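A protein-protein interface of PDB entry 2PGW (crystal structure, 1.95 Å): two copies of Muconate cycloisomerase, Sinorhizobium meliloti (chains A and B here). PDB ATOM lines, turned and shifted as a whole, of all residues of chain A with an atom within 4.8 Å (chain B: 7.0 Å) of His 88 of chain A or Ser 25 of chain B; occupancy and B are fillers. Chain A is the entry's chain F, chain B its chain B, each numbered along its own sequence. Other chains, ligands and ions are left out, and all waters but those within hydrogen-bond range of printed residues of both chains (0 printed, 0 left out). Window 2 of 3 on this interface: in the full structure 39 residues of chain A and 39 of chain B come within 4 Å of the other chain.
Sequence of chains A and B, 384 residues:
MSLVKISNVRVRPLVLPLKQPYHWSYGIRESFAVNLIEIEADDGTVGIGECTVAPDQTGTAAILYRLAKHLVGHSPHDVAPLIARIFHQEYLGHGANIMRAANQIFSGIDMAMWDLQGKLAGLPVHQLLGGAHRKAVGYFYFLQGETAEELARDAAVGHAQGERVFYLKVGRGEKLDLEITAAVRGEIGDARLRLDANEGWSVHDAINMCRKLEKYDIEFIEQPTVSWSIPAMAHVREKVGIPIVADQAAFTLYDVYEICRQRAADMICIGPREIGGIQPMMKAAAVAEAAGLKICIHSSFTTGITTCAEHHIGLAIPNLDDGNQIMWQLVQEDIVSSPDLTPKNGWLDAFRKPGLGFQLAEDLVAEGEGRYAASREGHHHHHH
No position is printed for both chains.
OH of Tyr 26 of chain B is in hydrogen-bond range of ND1 of His 88 of chain A, 2.9 Å away. The guanidinium group (NH2) of Arg 29 of chain B lies within hydrogen-bond range of the backbone carbonyl oxygen (O) of Gly 93 of chain A (2.9 Å).
Tyr 26 of chain B touches Arg 85 of chain A. Ser 25 of chain B touches His 88 of chain A (OG to CE1, 3.4 Å). O of Gln 89 of chain A touches CZ3 of Trp 24 of chain B, 3.3 Å away. Gln 89 of chain A touches Tyr 26 of chain B. Trp 24 of chain B touches Gly 93 of chain A (CE3 to CA, 3.9 Å).
Of the 10 printed residues of chain A, 4 touch a printed residue of chain B. Hydrophobic or aromatic side chains of chain A that line the printed part of chain B: His 88. Printed residues of chain B that touch a printed residue of chain A: Trp 24, Ser 25, Tyr 26 and Arg 29. Hydrophobic or aromatic side chains of chain B within 4 Å of the printed part of chain A: Trp 24 and Tyr 26. Among the printed residues, 7 pairs touch across the chains. Among the printed residues, no Asp or Glu carboxylate lies within 4 Å of a Lys or Arg side-chain nitrogen of the other chain.
Of chain B, only Ser 25 (3.4 Å) and Tyr 26 (2.9 Å) come within 4 Å of His 88 of chain A. Ser 25 of chain B touches just one residue of chain A: His 88 (3.4 Å). Printed residues of chain B within 4 Å of Gly 93 of chain A: Trp 24 (3.9 Å) and Arg 29 (2.9 Å). Of the printed residues of chain A, Trp 24 of chain B touches Gln 89 (3.3 Å) and Gly 93 (3.9 Å). Printed residues of chain B within 4 Å of Arg 85 of chain A: Tyr 26 (3.5 Å). Lys 169 of chain B touches none of the printed residues of chain A. The nearest residue of chain B that does not touch His 88 of chain A is Trp 24 of chain B (4.8 Å). The nearest printed residue of chain B that does not touch Arg 85 of chain A is Trp 24 of chain B (7.8 Å).
OE1 of Gln 89 of chain A sits at hydrogen-bond distance from NH1 of Arg 85 of chain A, at 2.5 Å. O of His 88 of chain A sits at hydrogen-bond distance from N of Gly 93 of chain A.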
ATOM      1  N   ALA A  84      12.256 -19.764   9.830  1.00  0.00           N
ATOM      2  CA  ALA A  84      11.491 -19.264  10.968  1.00  0.00           C
ATOM      3  C   ALA A  84      12.417 -18.843  12.101  1.00  0.00           C
ATOM      4  O   ALA A  84      12.207 -17.811  12.729  1.00  0.00           O
ATOM      5  CB  ALA A  84      10.524 -20.324  11.467  1.00  0.00           C
ATOM      6  N   ARG A  85      13.438 -19.660  12.354  1.00  0.00           N
ATOM      7  CA  ARG A  85      14.391 -19.370  13.416  1.00  0.00           C
ATOM      8  C   ARG A  85      15.213 -18.134  13.084  1.00  0.00           C
ATOM      9  O   ARG A  85      15.405 -17.270  13.937  1.00  0.00           O
ATOM     10  CB  ARG A  85      15.329 -20.563  13.634  1.00  0.00           C
ATOM     11  CG  ARG A  85      16.264 -20.390  14.832  1.00  0.00           C
ATOM     12  CD  ARG A  85      17.315 -21.493  14.895  1.00  0.00           C
ATOM     13  NE  ARG A  85      18.303 -21.381  13.821  1.00  0.00           N
ATOM     14  CZ  ARG A  85      19.220 -20.418  13.739  1.00  0.00           C
ATOM     15  NH1 ARG A  85      19.284 -19.475  14.669  1.00  0.00           N
ATOM     16  NH2 ARG A  85      20.078 -20.399  12.727  1.00  0.00           N
ATOM     17  N   ILE A  86      15.691 -18.051  11.841  1.00  0.00           N
ATOM     18  CA  ILE A  86      16.499 -16.910  11.410  1.00  0.00           C
ATOM     19  C   ILE A  86      15.678 -15.632  11.512  1.00  0.00           C
ATOM     20  O   ILE A  86      16.173 -14.594  11.969  1.00  0.00           O
ATOM     21  CB  ILE A  86      17.001 -17.095   9.942  1.00  0.00           C
ATOM     22  CG1 ILE A  86      17.879 -18.351   9.849  1.00  0.00           C
ATOM     23  CG2 ILE A  86      17.789 -15.857   9.478  1.00  0.00           C
ATOM     24  CD1 ILE A  86      18.217 -18.761   8.428  1.00  0.00           C
ATOM     25  N   PHE A  87      14.417 -15.708  11.091  1.00  0.00           N
ATOM     26  CA  PHE A  87      13.520 -14.561  11.142  1.00  0.00           C
ATOM     27  C   PHE A  87      13.370 -14.092  12.592  1.00  0.00           C
ATOM     28  O   PHE A  87      13.468 -12.898  12.879  1.00  0.00           O
ATOM     29  CB  PHE A  87      12.154 -14.952  10.556  1.00  0.00           C
ATOM     30  CG  PHE A  87      11.137 -13.838  10.560  1.00  0.00           C
ATOM     31  CD1 PHE A  87      11.475 -12.550  10.131  1.00  0.00           C
ATOM     32  CD2 PHE A  87       9.822 -14.093  10.960  1.00  0.00           C
ATOM     33  CE1 PHE A  87      10.517 -11.532  10.104  1.00  0.00           C
ATOM     34  CE2 PHE A  87       8.857 -13.088  10.941  1.00  0.00           C
ATOM     35  CZ  PHE A  87       9.201 -11.803  10.512  1.00  0.00           C
ATOM     36  N   HIS A  88      13.162 -15.039  13.499  1.00  0.00           N
ATOM     37  CA  HIS A  88      12.989 -14.721  14.911  1.00  0.00           C
ATOM     38  C   HIS A  88      14.245 -14.131  15.550  1.00  0.00           C
ATOM     39  O   HIS A  88      14.166 -13.163  16.296  1.00  0.00           O
ATOM     40  CB  HIS A  88      12.567 -15.977  15.689  1.00  0.00           C
ATOM     41  CG  HIS A  88      12.180 -15.707  17.110  1.00  0.00           C
ATOM     42  ND1 HIS A  88      12.425 -16.598  18.134  1.00  0.00           N
ATOM     43  CD2 HIS A  88      11.549 -14.650  17.679  1.00  0.00           C
ATOM     44  CE1 HIS A  88      11.969 -16.100  19.272  1.00  0.00           C
ATOM     45  NE2 HIS A  88      11.432 -14.919  19.023  1.00  0.00           N
ATOM     46  N   GLN A  89      15.404 -14.706  15.242  1.00  0.00           N
ATOM     47  CA  GLN A  89      16.665 -14.254  15.823  1.00  0.00           C
ATOM     48  C   GLN A  89      17.179 -12.923  15.291  1.00  0.00           C
ATOM     49  O   GLN A  89      17.583 -12.055  16.063  1.00  0.00           O
ATOM     50  CB  GLN A  89      17.746 -15.319  15.616  1.00  0.00           C
ATOM     51  CG  GLN A  89      19.018 -15.094  16.419  1.00  0.00           C
ATOM     52  CD  GLN A  89      20.118 -16.070  16.056  1.00  0.00           C
ATOM     53  OE1 GLN A  89      19.849 -17.166  15.565  1.00  0.00           O
ATOM     54  NE2 GLN A  89      21.364 -15.684  16.313  1.00  0.00           N
ATOM     55  N   GLU A  90      17.149 -12.764  13.967  1.00  0.00           N
ATOM     56  CA  GLU A  90      17.664 -11.568  13.326  1.00  0.00           C
ATOM     57  C   GLU A  90      16.694 -10.405  13.197  1.00  0.00           C
ATOM     58  O   GLU A  90      17.124  -9.266  13.066  1.00  0.00           O
ATOM     59  CB  GLU A  90      18.215 -11.928  11.941  1.00  0.00           C
ATOM     60  CG  GLU A  90      19.392 -12.909  11.982  1.00  0.00           C
ATOM     61  CD  GLU A  90      20.699 -12.253  12.400  1.00  0.00           C
ATOM     62  OE1 GLU A  90      20.659 -11.321  13.233  1.00  0.00           O
ATOM     63  OE2 GLU A  90      21.769 -12.680  11.905  1.00  0.00           O
ATOM     64  N   TYR A  91      15.394 -10.683  13.234  1.00  0.00           N
ATOM     65  CA  TYR A  91      14.396  -9.624  13.103  1.00  0.00           C
ATOM     66  C   TYR A  91      13.547  -9.421  14.356  1.00  0.00           C
ATOM     67  O   TYR A  91      13.652  -8.403  15.035  1.00  0.00           O
ATOM     68  CB  TYR A  91      13.460  -9.924  11.926  1.00  0.00           C
ATOM     69  CG  TYR A  91      14.071  -9.804  10.548  1.00  0.00           C
ATOM     70  CD1 TYR A  91      13.952  -8.621   9.807  1.00  0.00           C
ATOM     71  CD2 TYR A  91      14.714 -10.892   9.955  1.00  0.00           C
ATOM     72  CE1 TYR A  91      14.456  -8.536   8.504  1.00  0.00           C
ATOM     73  CE2 TYR A  91      15.220 -10.817   8.658  1.00  0.00           C
ATOM     74  CZ  TYR A  91      15.086  -9.641   7.942  1.00  0.00           C
ATOM     75  OH  TYR A  91      15.580  -9.575   6.665  1.00  0.00           O
ATOM     76  N   LEU A  92      12.700 -10.398  14.662  1.00  0.00           N
ATOM     77  CA  LEU A  92      11.796 -10.298  15.804  1.00  0.00           C
ATOM     78  C   LEU A  92      12.472 -10.069  17.158  1.00  0.00           C
ATOM     79  O   LEU A  92      11.956  -9.327  17.990  1.00  0.00           O
ATOM     80  CB  LEU A  92      10.900 -11.543  15.863  1.00  0.00           C
ATOM     81  CG  LEU A  92      10.157 -11.879  14.558  1.00  0.00           C
ATOM     82  CD1 LEU A  92       9.190 -13.031  14.807  1.00  0.00           C
ATOM     83  CD2 LEU A  92       9.397 -10.647  14.043  1.00  0.00           C
ATOM     84  N   GLY A  93      13.623 -10.695  17.375  1.00  0.00           N
ATOM     85  CA  GLY A  93      14.315 -10.527  18.642  1.00  0.00           C
ATOM     86  C   GLY A  93      14.833  -9.113  18.866  1.00  0.00           C
ATOM     87  O   GLY A  93      15.273  -8.777  19.959  1.00  0.00           O
ATOM     88  N   HIS B  23      18.728 -10.303  28.633  1.00  0.00           N
ATOM     89  CA  HIS B  23      18.283 -11.625  28.213  1.00  0.00           C
ATOM     90  C   HIS B  23      17.181 -11.624  27.162  1.00  0.00           C
ATOM     91  O   HIS B  23      16.178 -10.929  27.302  1.00  0.00           O
ATOM     92  CB  HIS B  23      17.817 -12.430  29.426  1.00  0.00           C
ATOM     93  CG  HIS B  23      18.924 -12.784  30.367  1.00  0.00           C
ATOM     94  ND1 HIS B  23      19.518 -11.859  31.199  1.00  0.00           N
ATOM     95  CD2 HIS B  23      19.575 -13.954  30.574  1.00  0.00           C
ATOM     96  CE1 HIS B  23      20.490 -12.443  31.879  1.00  0.00           C
ATOM     97  NE2 HIS B  23      20.544 -13.712  31.518  1.00  0.00           N
ATOM     98  N   TRP B  24      17.386 -12.412  26.107  1.00  0.00           N
ATOM     99  CA  TRP B  24      16.403 -12.537  25.037  1.00  0.00           C
ATOM    100  C   TRP B  24      16.318 -13.974  24.532  1.00  0.00           C
ATOM    101  O   TRP B  24      17.077 -14.845  24.963  1.00  0.00           O
ATOM    102  CB  TRP B  24      16.724 -11.584  23.878  1.00  0.00           C
ATOM    103  CG  TRP B  24      18.005 -11.855  23.155  1.00  0.00           C
ATOM    104  CD1 TRP B  24      19.263 -11.921  23.694  1.00  0.00           C
ATOM    105  CD2 TRP B  24      18.166 -12.029  21.744  1.00  0.00           C
ATOM    106  NE1 TRP B  24      20.194 -12.119  22.701  1.00  0.00           N
ATOM    107  CE2 TRP B  24      19.550 -12.189  21.494  1.00  0.00           C
ATOM    108  CE3 TRP B  24      17.274 -12.061  20.658  1.00  0.00           C
ATOM    109  CZ2 TRP B  24      20.065 -12.376  20.205  1.00  0.00           C
ATOM    110  CZ3 TRP B  24      17.788 -12.249  19.372  1.00  0.00           C
ATOM    111  CH2 TRP B  24      19.172 -12.404  19.161  1.00  0.00           C
ATOM    112  N   SER B  25      15.381 -14.201  23.620  1.00  0.00           N
ATOM    113  CA  SER B  25      15.135 -15.513  23.033  1.00  0.00           C
ATOM    114  C   SER B  25      16.391 -16.268  22.611  1.00  0.00           C
ATOM    115  O   SER B  25      16.429 -17.496  22.661  1.00  0.00           O
ATOM    116  CB  SER B  25      14.218 -15.363  21.819  1.00  0.00           C
ATOM    117  OG  SER B  25      13.086 -14.571  22.133  1.00  0.00           O
ATOM    118  N   TYR B  26      17.418 -15.539  22.192  1.00  0.00           N
ATOM    119  CA  TYR B  26      18.642 -16.184  21.747  1.00  0.00           C
ATOM    120  C   TYR B  26      19.862 -15.898  22.604  1.00  0.00           C
ATOM    121  O   TYR B  26      20.931 -15.557  22.098  1.00  0.00           O
ATOM    122  CB  TYR B  26      18.891 -15.821  20.284  1.00  0.00           C
ATOM    123  CG  TYR B  26      17.817 -16.404  19.401  1.00  0.00           C
ATOM    124  CD1 TYR B  26      17.935 -17.703  18.899  1.00  0.00           C
ATOM    125  CD2 TYR B  26      16.635 -15.703  19.151  1.00  0.00           C
ATOM    126  CE1 TYR B  26      16.902 -18.296  18.175  1.00  0.00           C
ATOM    127  CE2 TYR B  26      15.588 -16.285  18.431  1.00  0.00           C
ATOM    128  CZ  TYR B  26      15.729 -17.584  17.947  1.00  0.00           C
ATOM    129  OH  TYR B  26      14.697 -18.184  17.253  1.00  0.00           O
ATOM    130  N   GLY B  27      19.685 -16.038  23.915  1.00  0.00           N
ATOM    131  CA  GLY B  27      20.786 -15.836  24.834  1.00  0.00           C
ATOM    132  C   GLY B  27      20.907 -14.507  25.548  1.00  0.00           C
ATOM    133  O   GLY B  27      19.976 -14.029  26.195  1.00  0.00           O
ATOM    134  N   ILE B  28      22.083 -13.910  25.416  1.00  0.00           N
ATOM    135  CA  ILE B  28      22.381 -12.655  26.071  1.00  0.00           C
ATOM    136  C   ILE B  28      22.878 -11.593  25.102  1.00  0.00           C
ATOM    137  O   ILE B  28      23.632 -11.875  24.172  1.00  0.00           O
ATOM    138  CB  ILE B  28      23.443 -12.892  27.164  1.00  0.00           C
ATOM    139  CG1 ILE B  28      22.860 -13.800  28.252  1.00  0.00           C
ATOM    140  CG2 ILE B  28      23.927 -11.572  27.724  1.00  0.00           C
ATOM    141  CD1 ILE B  28      23.880 -14.334  29.232  1.00  0.00           C
ATOM    142  N   ARG B  29      22.433 -10.365  25.334  1.00  0.00           N
ATOM    143  CA  ARG B  29      22.822  -9.219  24.528  1.00  0.00           C
ATOM    144  C   ARG B  29      23.570  -8.304  25.491  1.00  0.00           C
ATOM    145  O   ARG B  29      22.986  -7.766  26.425  1.00  0.00           O
ATOM    146  CB  ARG B  29      21.569  -8.530  23.983  1.00  0.00           C
ATOM    147  CG  ARG B  29      21.819  -7.284  23.154  1.00  0.00           C
ATOM    148  CD  ARG B  29      20.500  -6.730  22.642  1.00  0.00           C
ATOM    149  NE  ARG B  29      19.873  -7.653  21.703  1.00  0.00           N
ATOM    150  CZ  ARG B  29      18.560  -7.830  21.587  1.00  0.00           C
ATOM    151  NH1 ARG B  29      17.728  -7.150  22.359  1.00  0.00           N
ATOM    152  NH2 ARG B  29      18.082  -8.684  20.689  1.00  0.00           N
ATOM    153  N   LYS B 169       7.837  -8.470  32.343  1.00  0.00           N
ATOM    154  CA  LYS B 169       7.744  -9.366  31.204  1.00  0.00           C
ATOM    155  C   LYS B 169       7.311 -10.768  31.641  1.00  0.00           C
ATOM    156  O   LYS B 169       7.909 -11.358  32.535  1.00  0.00           O
ATOM    157  CB  LYS B 169       9.095  -9.418  30.491  1.00  0.00           C
ATOM    158  CG  LYS B 169       9.201 -10.440  29.371  1.00  0.00           C
ATOM    159  CD  LYS B 169      10.531 -10.291  28.631  1.00  0.00           C
ATOM    160  CE  LYS B 169      10.695 -11.319  27.520  1.00  0.00           C
ATOM    161  NZ  LYS B 169      10.769 -12.713  28.045  1.00  0.00           N
ATOM    162  N   ASN B 198       4.586 -10.218  25.304  1.00  0.00           N
ATOM    163  CA  ASN B 198       5.507 -10.261  24.171  1.00  0.00           C
ATOM    164  C   ASN B 198       5.182 -11.279  23.058  1.00  0.00           C
ATOM    165  O   ASN B 198       6.040 -12.077  22.679  1.00  0.00           O
ATOM    166  CB  ASN B 198       6.908 -10.515  24.743  1.00  0.00           C
ATOM    167  CG  ASN B 198       8.012 -10.300  23.725  1.00  0.00           C
ATOM    168  OD1 ASN B 198       7.972  -9.353  22.937  1.00  0.00           O
ATOM    169  ND2 ASN B 198       9.017 -11.174  23.753  1.00  0.00           N
